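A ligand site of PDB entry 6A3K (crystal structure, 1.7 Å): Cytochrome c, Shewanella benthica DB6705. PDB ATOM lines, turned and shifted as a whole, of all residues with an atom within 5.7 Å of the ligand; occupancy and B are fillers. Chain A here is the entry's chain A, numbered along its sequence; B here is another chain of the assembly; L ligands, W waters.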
ATOM      1  N   ILE A  10       4.257  11.457  17.755  1.00  0.00           N
ATOM      2  CA  ILE A  10       4.268  10.033  18.078  1.00  0.00           C
ATOM      3  C   ILE A  10       3.094   9.667  18.969  1.00  0.00           C
ATOM      4  O   ILE A  10       2.373   8.691  18.725  1.00  0.00           O
ATOM      5  CB  ILE A  10       5.609   9.668  18.734  1.00  0.00           C
ATOM      6  CG1 ILE A  10       6.748   9.815  17.710  1.00  0.00           C
ATOM      7  CG2 ILE A  10       5.567   8.264  19.337  1.00  0.00           C
ATOM      8  CD1 ILE A  10       8.154   9.743  18.360  1.00  0.00           C
ATOM      9  N   ARG A  13      -0.302   9.690  16.850  1.00  0.00           N
ATOM     10  CA  ARG A  13      -0.569   8.525  15.998  1.00  0.00           C
ATOM     11  C   ARG A  13      -0.757   7.258  16.829  1.00  0.00           C
ATOM     12  O   ARG A  13      -1.645   6.456  16.556  1.00  0.00           O
ATOM     13  CB  ARG A  13       0.532   8.363  14.947  1.00  0.00           C
ATOM     14  CG  ARG A  13       1.929   7.979  15.474  1.00  0.00           C
ATOM     15  CD  ARG A  13       3.032   8.480  14.526  1.00  0.00           C
ATOM     16  NE  ARG A  13       4.345   7.890  14.810  1.00  0.00           N
ATOM     17  CZ  ARG A  13       5.515   8.438  14.472  1.00  0.00           C
ATOM     18  NH1 ARG A  13       5.538   9.618  13.871  1.00  0.00           N
ATOM     19  NH2 ARG A  13       6.663   7.806  14.736  1.00  0.00           N
ATOM     20  N   GLN A  14       0.068   7.083  17.874  1.00  0.00           N
ATOM     21  CA  GLN A  14      -0.108   5.923  18.732  1.00  0.00           C
ATOM     22  C   GLN A  14      -1.493   5.916  19.378  1.00  0.00           C
ATOM     23  O   GLN A  14      -2.148   4.870  19.442  1.00  0.00           O
ATOM     24  CB  GLN A  14       0.977   5.887  19.803  1.00  0.00           C
ATOM     25  CG  GLN A  14       2.337   5.520  19.254  1.00  0.00           C
ATOM     26  CD  GLN A  14       3.401   5.496  20.321  1.00  0.00           C
ATOM     27  OE1 GLN A  14       3.226   6.087  21.393  1.00  0.00           O
ATOM     28  NE2 GLN A  14       4.514   4.813  20.044  1.00  0.00           N
ATOM     29  N   SER A  15      -1.966   7.068  19.845  1.00  0.00           N
ATOM     30  CA  SER A  15      -3.288   7.102  20.473  1.00  0.00           C
ATOM     31  C   SER A  15      -4.385   6.760  19.469  1.00  0.00           C
ATOM     32  O   SER A  15      -5.326   6.040  19.811  1.00  0.00           O
ATOM     33  CB  SER A  15      -3.540   8.473  21.091  1.00  0.00           C
ATOM     34  OG  SER A  15      -2.714   8.657  22.232  1.00  0.00           O
ATOM     35  N   PHE A  17      -4.161   4.885  16.755  1.00  0.00           N
ATOM     36  CA  PHE A  17      -4.108   3.444  16.502  1.00  0.00           C
ATOM     37  C   PHE A  17      -4.688   2.650  17.661  1.00  0.00           C
ATOM     38  O   PHE A  17      -5.420   1.676  17.461  1.00  0.00           O
ATOM     39  CB  PHE A  17      -2.667   3.017  16.262  1.00  0.00           C
ATOM     40  CG  PHE A  17      -2.137   3.401  14.913  1.00  0.00           C
ATOM     41  CD1 PHE A  17      -2.832   3.104  13.751  1.00  0.00           C
ATOM     42  CD2 PHE A  17      -0.907   4.046  14.807  1.00  0.00           C
ATOM     43  CE1 PHE A  17      -2.310   3.457  12.512  1.00  0.00           C
ATOM     44  CE2 PHE A  17      -0.399   4.388  13.582  1.00  0.00           C
ATOM     45  CZ  PHE A  17      -1.101   4.089  12.426  1.00  0.00           C
ATOM     46  N   SER A  18      -4.348   3.029  18.895  1.00  0.00           N
ATOM     47  CA  SER A  18      -4.877   2.313  20.058  1.00  0.00           C
ATOM     48  C   SER A  18      -6.397   2.374  20.090  1.00  0.00           C
ATOM     49  O   SER A  18      -7.068   1.357  20.333  1.00  0.00           O
ATOM     50  CB  SER A  18      -4.266   2.897  21.337  1.00  0.00           C
ATOM     51  OG  SER A  18      -4.807   2.275  22.490  1.00  0.00           O
ATOM     52  N   MET A  20      -8.356   2.834  17.520  1.00  0.00           N
ATOM     53  CA  MET A  20      -8.800   2.011  16.395  1.00  0.00           C
ATOM     54  C   MET A  20      -8.857   0.546  16.786  1.00  0.00           C
ATOM     55  O   MET A  20      -9.829  -0.157  16.492  1.00  0.00           O
ATOM     56  CB  MET A  20      -7.856   2.178  15.199  1.00  0.00           C
ATOM     57  CG  MET A  20      -7.921   3.501  14.500  1.00  0.00           C
ATOM     58  SD  MET A  20      -6.485   3.861  13.479  1.00  0.00           S
ATOM     59  CE  MET A  20      -6.492   2.488  12.327  1.00  0.00           C
ATOM     60  N   ALA A  21      -7.801   0.077  17.453  1.00  0.00           N
ATOM     61  CA  ALA A  21      -7.722  -1.331  17.839  1.00  0.00           C
ATOM     62  C   ALA A  21      -8.828  -1.703  18.804  1.00  0.00           C
ATOM     63  O   ALA A  21      -9.394  -2.806  18.722  1.00  0.00           O
ATOM     64  CB  ALA A  21      -6.355  -1.635  18.433  1.00  0.00           C
ATOM     65  N   PHE A  24     -12.015  -1.873  16.588  1.00  0.00           N
ATOM     66  CA  PHE A  24     -11.912  -2.970  15.619  1.00  0.00           C
ATOM     67  C   PHE A  24     -11.983  -4.327  16.312  1.00  0.00           C
ATOM     68  O   PHE A  24     -12.620  -5.266  15.796  1.00  0.00           O
ATOM     69  CB  PHE A  24     -10.610  -2.842  14.835  1.00  0.00           C
ATOM     70  CG  PHE A  24     -10.559  -3.693  13.598  1.00  0.00           C
ATOM     71  CD1 PHE A  24     -11.481  -3.499  12.577  1.00  0.00           C
ATOM     72  CD2 PHE A  24      -9.579  -4.672  13.467  1.00  0.00           C
ATOM     73  CE1 PHE A  24     -11.437  -4.284  11.425  1.00  0.00           C
ATOM     74  CE2 PHE A  24      -9.528  -5.459  12.322  1.00  0.00           C
ATOM     75  CZ  PHE A  24     -10.457  -5.253  11.296  1.00  0.00           C
ATOM     76  N   VAL A  49     -14.264   3.154  13.703  1.00  0.00           N
ATOM     77  CA  VAL A  49     -13.034   2.757  13.019  1.00  0.00           C
ATOM     78  C   VAL A  49     -12.805   3.602  11.767  1.00  0.00           C
ATOM     79  O   VAL A  49     -11.681   3.977  11.443  1.00  0.00           O
ATOM     80  CB  VAL A  49     -13.072   1.253  12.688  1.00  0.00           C
ATOM     81  CG1 VAL A  49     -11.936   0.881  11.718  1.00  0.00           C
ATOM     82  CG2 VAL A  49     -12.964   0.459  13.981  1.00  0.00           C
ATOM     83  N   PHE A  60       2.758  11.197  11.190  1.00  0.00           N
ATOM     84  CA  PHE A  60       4.015  10.681  10.648  1.00  0.00           C
ATOM     85  C   PHE A  60       4.828  11.808  10.007  1.00  0.00           C
ATOM     86  O   PHE A  60       5.130  11.805   8.815  1.00  0.00           O
ATOM     87  CB  PHE A  60       3.749   9.526   9.689  1.00  0.00           C
ATOM     88  CG  PHE A  60       3.292   8.283  10.389  1.00  0.00           C
ATOM     89  CD1 PHE A  60       4.223   7.352  10.831  1.00  0.00           C
ATOM     90  CD2 PHE A  60       1.948   8.062  10.646  1.00  0.00           C
ATOM     91  CE1 PHE A  60       3.808   6.207  11.490  1.00  0.00           C
ATOM     92  CE2 PHE A  60       1.526   6.918  11.298  1.00  0.00           C
ATOM     93  CZ  PHE A  60       2.456   5.989  11.726  1.00  0.00           C
ATOM     94  N   GLU A  68      10.830   6.988  21.474  1.00  0.00           N
ATOM     95  CA  GLU A  68       9.954   5.888  21.872  1.00  0.00           C
ATOM     96  C   GLU A  68       8.845   5.704  20.840  1.00  0.00           C
ATOM     97  O   GLU A  68       7.683   6.055  21.051  1.00  0.00           O
ATOM     98  CB  GLU A  68       9.380   6.159  23.266  1.00  0.00           C
ATOM     99  CG  GLU A  68       8.926   4.918  24.010  1.00  0.00           C
ATOM    100  CD  GLU A  68      10.091   4.044  24.428  1.00  0.00           C
ATOM    101  OE1 GLU A  68      11.123   4.608  24.851  1.00  0.00           O
ATOM    102  OE2 GLU A  68       9.967   2.807  24.318  1.00  0.00           O
ATOM    103  N   THR A  69       9.206   5.085  19.716  1.00  0.00           N
ATOM    104  CA  THR A  69       8.248   4.811  18.645  1.00  0.00           C
ATOM    105  C   THR A  69       8.571   3.474  18.001  1.00  0.00           C
ATOM    106  O   THR A  69       9.732   3.054  17.943  1.00  0.00           O
ATOM    107  CB  THR A  69       8.261   5.916  17.576  1.00  0.00           C
ATOM    108  OG1 THR A  69       7.344   5.567  16.517  1.00  0.00           O
ATOM    109  CG2 THR A  69       9.654   6.107  16.979  1.00  0.00           C
ATOM    110  N   GLU A  70       7.518   2.797  17.529  1.00  0.00           N
ATOM    111  CA  GLU A  70       7.644   1.561  16.763  1.00  0.00           C
ATOM    112  C   GLU A  70       7.551   1.782  15.261  1.00  0.00           C
ATOM    113  O   GLU A  70       7.437   0.819  14.495  1.00  0.00           O
ATOM    114  CB  GLU A  70       6.597   0.547  17.222  1.00  0.00           C
ATOM    115  CG  GLU A  70       6.639   0.289  18.714  1.00  0.00           C
ATOM    116  CD  GLU A  70       7.991  -0.252  19.163  1.00  0.00           C
ATOM    117  OE1 GLU A  70       8.401  -1.315  18.666  1.00  0.00           O
ATOM    118  OE2 GLU A  70       8.642   0.378  20.023  1.00  0.00           O
ATOM    119  N   ALA A  71       7.606   3.035  14.809  1.00  0.00           N
ATOM    120  CA  ALA A  71       7.590   3.320  13.386  1.00  0.00           C
ATOM    121  C   ALA A  71       8.992   3.208  12.832  1.00  0.00           C
ATOM    122  O   ALA A  71       9.926   3.807  13.361  1.00  0.00           O
ATOM    123  CB  ALA A  71       7.038   4.720  13.140  1.00  0.00           C
ATOM    124  N   LEU A  72       9.147   2.435  11.756  1.00  0.00           N
ATOM    125  CA  LEU A  72      10.444   2.270  11.126  1.00  0.00           C
ATOM    126  C   LEU A  72      10.829   3.497  10.305  1.00  0.00           C
ATOM    127  O   LEU A  72       9.978   4.135   9.673  1.00  0.00           O
ATOM    128  CB  LEU A  72      10.456   1.041  10.231  1.00  0.00           C
ATOM    129  CG  LEU A  72      10.396  -0.287  10.979  1.00  0.00           C
ATOM    130  CD1 LEU A  72      10.060  -1.386  10.006  1.00  0.00           C
ATOM    131  CD2 LEU A  72      11.714  -0.578  11.679  1.00  0.00           C
ATOM    132  N   ILE A  75       9.614   4.258   6.675  1.00  0.00           N
ATOM    133  CA  ILE A  75       8.350   4.915   6.351  1.00  0.00           C
ATOM    134  C   ILE A  75       8.624   6.175   5.542  1.00  0.00           C
ATOM    135  O   ILE A  75       7.894   6.501   4.592  1.00  0.00           O
ATOM    136  CB  ILE A  75       7.565   5.236   7.630  1.00  0.00           C
ATOM    137  CG1 ILE A  75       7.009   3.954   8.234  1.00  0.00           C
ATOM    138  CG2 ILE A  75       6.447   6.248   7.343  1.00  0.00           C
ATOM    139  CD1 ILE A  75       6.440   4.142   9.635  1.00  0.00           C
ATOM    140  N   PHE A  82       3.712   3.945   1.832  1.00  0.00           N
ATOM    141  CA  PHE A  82       3.085   4.009   3.147  1.00  0.00           C
ATOM    142  C   PHE A  82       1.760   4.736   3.063  1.00  0.00           C
ATOM    143  O   PHE A  82       0.737   4.262   3.572  1.00  0.00           O
ATOM    144  CB  PHE A  82       4.001   4.704   4.149  1.00  0.00           C
ATOM    145  CG  PHE A  82       3.457   4.747   5.564  1.00  0.00           C
ATOM    146  CD1 PHE A  82       3.637   3.665   6.417  1.00  0.00           C
ATOM    147  CD2 PHE A  82       2.786   5.875   6.037  1.00  0.00           C
ATOM    148  CE1 PHE A  82       3.166   3.703   7.733  1.00  0.00           C
ATOM    149  CE2 PHE A  82       2.293   5.904   7.346  1.00  0.00           C
ATOM    150  CZ  PHE A  82       2.479   4.824   8.191  1.00  0.00           C
ATOM    151  N   LYS A  85      -0.904   2.612   1.444  1.00  0.00           N
ATOM    152  CA  LYS A  85      -1.504   1.641   2.354  1.00  0.00           C
ATOM    153  C   LYS A  85      -2.499   2.318   3.294  1.00  0.00           C
ATOM    154  O   LYS A  85      -3.558   1.753   3.593  1.00  0.00           O
ATOM    155  CB  LYS A  85      -0.418   0.921   3.160  1.00  0.00           C
ATOM    156  CG  LYS A  85       0.370  -0.149   2.352  1.00  0.00           C
ATOM    157  CD  LYS A  85       1.376  -0.872   3.248  1.00  0.00           C
ATOM    158  CE  LYS A  85       2.310  -1.754   2.438  1.00  0.00           C
ATOM    159  NZ  LYS A  85       1.574  -2.730   1.597  1.00  0.00           N
ATOM    160  N   MET A  86      -2.184   3.534   3.750  1.00  0.00           N
ATOM    161  CA  MET A  86      -3.118   4.216   4.651  1.00  0.00           C
ATOM    162  C   MET A  86      -4.401   4.575   3.912  1.00  0.00           C
ATOM    163  O   MET A  86      -5.499   4.413   4.455  1.00  0.00           O
ATOM    164  CB  MET A  86      -2.475   5.466   5.247  1.00  0.00           C
ATOM    165  CG  MET A  86      -3.230   6.003   6.449  1.00  0.00           C
ATOM    166  SD  MET A  86      -3.143   4.919   7.884  1.00  0.00           S
ATOM    167  CE  MET A  86      -1.616   5.456   8.627  1.00  0.00           C
ATOM    168  N   LEU A  89      -6.536   1.546   3.664  1.00  0.00           N
ATOM    169  CA  LEU A  89      -7.221   1.354   4.942  1.00  0.00           C
ATOM    170  C   LEU A  89      -8.501   2.166   4.993  1.00  0.00           C
ATOM    171  O   LEU A  89      -9.557   1.667   5.427  1.00  0.00           O
ATOM    172  CB  LEU A  89      -6.310   1.732   6.122  1.00  0.00           C
ATOM    173  CG  LEU A  89      -7.013   1.714   7.506  1.00  0.00           C
ATOM    174  CD1 LEU A  89      -7.421   0.298   7.925  1.00  0.00           C
ATOM    175  CD2 LEU A  89      -6.156   2.353   8.608  1.00  0.00           C
ATOM    176  N   VAL A 115     -10.221  -5.101   6.051  1.00  0.00           N
ATOM    177  CA  VAL A 115      -9.595  -4.108   6.930  1.00  0.00           C
ATOM    178  C   VAL A 115      -8.445  -4.741   7.698  1.00  0.00           C
ATOM    179  O   VAL A 115      -7.347  -4.170   7.801  1.00  0.00           O
ATOM    180  CB  VAL A 115     -10.634  -3.491   7.876  1.00  0.00           C
ATOM    181  CG1 VAL A 115      -9.940  -2.529   8.854  1.00  0.00           C
ATOM    182  CG2 VAL A 115     -11.711  -2.756   7.095  1.00  0.00           C
ATOM    183  N   ALA A 116      -8.675  -5.929   8.273  1.00  0.00           N
ATOM    184  CA  ALA A 116      -7.630  -6.583   9.064  1.00  0.00           C
ATOM    185  C   ALA A 116      -6.369  -6.801   8.232  1.00  0.00           C
ATOM    186  O   ALA A 116      -5.250  -6.684   8.746  1.00  0.00           O
ATOM    187  CB  ALA A 116      -8.126  -7.912   9.635  1.00  0.00           C
ATOM    188  N   SER A 118      -5.393  -4.871   5.866  1.00  0.00           N
ATOM    189  CA  SER A 118      -4.746  -3.559   5.796  1.00  0.00           C
ATOM    190  C   SER A 118      -3.878  -3.302   7.027  1.00  0.00           C
ATOM    191  O   SER A 118      -2.746  -2.832   6.901  1.00  0.00           O
ATOM    192  CB  SER A 118      -5.796  -2.455   5.652  1.00  0.00           C
ATOM    193  OG  SER A 118      -6.193  -2.290   4.300  1.00  0.00           O
ATOM    194  N   CYS A 119      -4.421  -3.564   8.219  1.00  0.00           N
ATOM    195  CA  CYS A 119      -3.641  -3.403   9.438  1.00  0.00           C
ATOM    196  C   CYS A 119      -2.368  -4.238   9.404  1.00  0.00           C
ATOM    197  O   CYS A 119      -1.261  -3.716   9.548  1.00  0.00           O
ATOM    198  CB  CYS A 119      -4.468  -3.786  10.681  1.00  0.00           C
ATOM    199  SG  CYS A 119      -6.192  -3.248  10.763  1.00  0.00           S
ATOM    200  N   CYS A 122       0.387  -3.367   6.574  1.00  0.00           N
ATOM    201  CA  CYS A 122       1.229  -2.222   6.872  1.00  0.00           C
ATOM    202  C   CYS A 122       2.197  -2.539   7.997  1.00  0.00           C
ATOM    203  O   CYS A 122       3.390  -2.220   7.903  1.00  0.00           O
ATOM    204  CB  CYS A 122       0.382  -1.002   7.213  1.00  0.00           C
ATOM    205  SG  CYS A 122       1.414   0.470   7.461  1.00  0.00           S
ATOM    206  N   HIS A 123       1.708  -3.169   9.073  1.00  0.00           N
ATOM    207  CA  HIS A 123       2.574  -3.532  10.196  1.00  0.00           C
ATOM    208  C   HIS A 123       3.737  -4.410   9.757  1.00  0.00           C
ATOM    209  O   HIS A 123       4.874  -4.218  10.190  1.00  0.00           O
ATOM    210  CB  HIS A 123       1.764  -4.263  11.279  1.00  0.00           C
ATOM    211  CG  HIS A 123       0.781  -3.401  11.986  1.00  0.00           C
ATOM    212  ND1 HIS A 123      -0.195  -3.916  12.816  1.00  0.00           N
ATOM    213  CD2 HIS A 123       0.619  -2.054  12.003  1.00  0.00           C
ATOM    214  CE1 HIS A 123      -0.926  -2.922  13.310  1.00  0.00           C
ATOM    215  NE2 HIS A 123      -0.458  -1.779  12.822  1.00  0.00           N
ATOM    216  N   TYR A 126       6.170  -1.887   7.904  1.00  0.00           N
ATOM    217  CA  TYR A 126       6.553  -0.556   8.385  1.00  0.00           C
ATOM    218  C   TYR A 126       6.586  -0.392   9.905  1.00  0.00           C
ATOM    219  O   TYR A 126       6.941   0.698  10.379  1.00  0.00           O
ATOM    220  CB  TYR A 126       5.616   0.496   7.792  1.00  0.00           C
ATOM    221  CG  TYR A 126       5.783   0.645   6.297  1.00  0.00           C
ATOM    222  CD1 TYR A 126       6.949   1.176   5.777  1.00  0.00           C
ATOM    223  CD2 TYR A 126       4.784   0.266   5.418  1.00  0.00           C
ATOM    224  CE1 TYR A 126       7.124   1.322   4.411  1.00  0.00           C
ATOM    225  CE2 TYR A 126       4.952   0.403   4.043  1.00  0.00           C
ATOM    226  CZ  TYR A 126       6.119   0.939   3.552  1.00  0.00           C
ATOM    227  OH  TYR A 126       6.295   1.075   2.185  1.00  0.00           O
ATOM    228  N   LYS A 127       6.231  -1.408  10.678  1.00  0.00           N
ATOM    229  CA  LYS A 127       6.294  -1.324  12.132  1.00  0.00           C
ATOM    230  C   LYS A 127       7.427  -2.222  12.627  1.00  0.00           C
ATOM    231  O   LYS A 127       7.629  -3.322  12.099  1.00  0.00           O
ATOM    232  CB  LYS A 127       4.960  -1.745  12.747  1.00  0.00           C
ATOM    233  CG  LYS A 127       4.858  -1.564  14.257  1.00  0.00           C
ATOM    234  CD  LYS A 127       3.425  -1.858  14.707  1.00  0.00           C
ATOM    235  CE  LYS A 127       3.232  -1.565  16.178  1.00  0.00           C
ATOM    236  NZ  LYS A 127       3.873  -2.610  17.019  1.00  0.00           N
ATOM    237  N   HIS B  11      -6.916   4.426  29.851  1.00  0.00           N
ATOM    238  CA  HIS B  11      -6.113   4.794  28.694  1.00  0.00           C
ATOM    239  C   HIS B  11      -6.990   5.170  27.509  1.00  0.00           C
ATOM    240  O   HIS B  11      -6.690   6.127  26.786  1.00  0.00           O
ATOM    241  CB  HIS B  11      -5.179   3.634  28.344  1.00  0.00           C
ATOM    242  CG  HIS B  11      -4.497   3.791  27.031  1.00  0.00           C
ATOM    243  ND1 HIS B  11      -3.346   4.529  26.881  1.00  0.00           N
ATOM    244  CD2 HIS B  11      -4.791   3.299  25.795  1.00  0.00           C
ATOM    245  CE1 HIS B  11      -2.949   4.494  25.620  1.00  0.00           C
ATOM    246  NE2 HIS B  11      -3.818   3.757  24.940  1.00  0.00           N
HETATM  247 FE1  LIG L   1      -1.233   0.193  13.099  1.00  0.00          FE
HETATM  248  C1  LIG L   1       0.913   1.125  15.698  1.00  0.00           C
HETATM  249  C2  LIG L   1      -3.491  -0.972  15.385  1.00  0.00           C
HETATM  250  C3  LIG L   1      -3.644  -0.040  10.625  1.00  0.00           C
HETATM  251  C4  LIG L   1       0.987   1.467  10.836  1.00  0.00           C
HETATM  252  N1  LIG L   1      -1.272   0.117  15.155  1.00  0.00           N
HETATM  253  C5  LIG L   1      -0.280   0.495  16.042  1.00  0.00           C
HETATM  254  C6  LIG L   1      -0.704   0.133  17.367  1.00  0.00           C
HETATM  255  C7  LIG L   1      -1.909  -0.446  17.276  1.00  0.00           C
HETATM  256  C8  LIG L   1      -2.306  -0.467  15.882  1.00  0.00           C
HETATM  257  C9  LIG L   1      -2.766  -0.987  18.440  1.00  0.00           C
HETATM  258  C10 LIG L   1       0.077   0.388  18.683  1.00  0.00           C
HETATM  259  C11 LIG L   1      -0.270   1.827  19.117  1.00  0.00           C
HETATM  260  C12 LIG L   1       0.394   2.187  20.437  1.00  0.00           C
HETATM  261  O1  LIG L   1      -0.309   2.142  21.477  1.00  0.00           O
HETATM  262  O2  LIG L   1       1.594   2.539  20.436  1.00  0.00           O
HETATM  263  N2  LIG L   1      -3.257  -0.337  13.019  1.00  0.00           N
HETATM  264  C13 LIG L   1      -3.930  -0.905  14.075  1.00  0.00           C
HETATM  265  C14 LIG L   1      -5.180  -1.434  13.555  1.00  0.00           C
HETATM  266  C15 LIG L   1      -5.221  -1.215  12.222  1.00  0.00           C
HETATM  267  C16 LIG L   1      -4.004  -0.483  11.874  1.00  0.00           C
HETATM  268  C17 LIG L   1      -6.209  -2.170  14.440  1.00  0.00           C
HETATM  269  C18 LIG L   1      -6.326  -1.533  11.201  1.00  0.00           C
HETATM  270  C19 LIG L   1      -7.619  -1.364  11.537  1.00  0.00           C
HETATM  271  N3  LIG L   1      -1.329   0.650  11.101  1.00  0.00           N
HETATM  272  C20 LIG L   1      -2.385   0.440  10.249  1.00  0.00           C
HETATM  273  C21 LIG L   1      -1.982   0.825   8.922  1.00  0.00           C
HETATM  274  C22 LIG L   1      -0.700   1.237   8.964  1.00  0.00           C
HETATM  275  C23 LIG L   1      -0.270   1.145  10.356  1.00  0.00           C
HETATM  276  C24 LIG L   1      -2.932   0.702   7.691  1.00  0.00           C
HETATM  277  C25 LIG L   1       0.238   1.744   7.853  1.00  0.00           C
HETATM  278  C26 LIG L   1      -0.249   2.167   6.663  1.00  0.00           C
HETATM  279  N4  LIG L   1       0.629   1.144  13.245  1.00  0.00           N
HETATM  280  C27 LIG L   1       1.375   1.552  12.163  1.00  0.00           C
HETATM  281  C28 LIG L   1       2.618   2.081  12.676  1.00  0.00           C
HETATM  282  C29 LIG L   1       2.598   1.996  14.016  1.00  0.00           C
HETATM  283  C30 LIG L   1       1.331   1.401  14.407  1.00  0.00           C
HETATM  284  C31 LIG L   1       3.762   2.639  11.801  1.00  0.00           C
HETATM  285  C32 LIG L   1       3.697   2.444  14.997  1.00  0.00           C
HETATM  286  C33 LIG L   1       3.338   3.853  15.483  1.00  0.00           C
HETATM  287  C34 LIG L   1       4.334   4.362  16.489  1.00  0.00           C
HETATM  288  O3  LIG L   1       4.745   3.578  17.392  1.00  0.00           O
HETATM  289  O4  LIG L   1       4.701   5.554  16.404  1.00  0.00           O
HETATM  290  O   HOH W   1       0.985   0.607  24.164  1.00  0.00           O
HETATM  291  O   HOH W   2       3.293   1.507  18.532  1.00  0.00           O
HETATM  292  O   HOH W   3       2.789   2.397  22.771  1.00  0.00           O
HETATM  293  O   HOH W   4      -1.363   3.956  23.160  1.00  0.00           O
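Water W4 bridges O1 of the ligand (2.7 Å) and NE2 of His 11 of chain B (3.0 Å).
A ring nitrogen (ND1) of His 123 lies close to the backbone carbonyl oxygen (O) of Cys 119 (3.4 Å).
NH2 of Arg 13 sits at hydrogen-bond distance from OG1 of Thr 69 (2.9 Å).
OG1 of Thr 69 sits at hydrogen-bond distance from N of Ala 71.
The backbone NH (N) of Leu 72 lies within hydrogen-bond range of the backbone carbonyl oxygen (O) of Tyr 126 (3.1 Å).
Merely in contact with the ligand: Phe 17, Met 20, Ala 21, Phe 60, Ala 71, Ile 75, Phe 82, Lys 85, Met 86, Leu 89, Val 115, Ser 118, Tyr 126 and Lys 127.
Hydrophobic or aromatic side chains that line the ligand: Phe 17, Met 20, Ala 21, Phe 60, Ile 75, Phe 82, Leu 89, Val 115 and His 123.
21 residues have an atom within 4 Å of the ligand: Arg 13, Gln 14, Phe 17, Met 20, Ala 21, Phe 60, Thr 69, Glu 70, Ala 71, Ile 75, Phe 82, Lys 85, Met 86, Leu 89, Val 115, Ser 118, Cys 119, Cys 122, His 123, Tyr 126 and Lys 127.
A carbon (C18) of the ligand is bonded to the side-chain sulfur (SG) of Cys 119 (1.8 Å).
SG of Cys 122 is covalently linked to C25 of the ligand.
A ring nitrogen (NE2) of His 123 binds an iron atom (FE1) of the ligand (2.1 Å).
OG1 of Thr 69 lies within hydrogen-bond range of O4 of the ligand (2.6 Å).
The guanidinium group (NE) of Arg 13 lies within salt-bridge range of an oxygen (O4) of the ligand (2.9 Å).
N of Glu 70 is in hydrogen-bond range of O3 of the ligand (2.9 Å).
O3 of the ligand lies within hydrogen-bond range of NE2 of Gln 14, at 2.9 Å.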
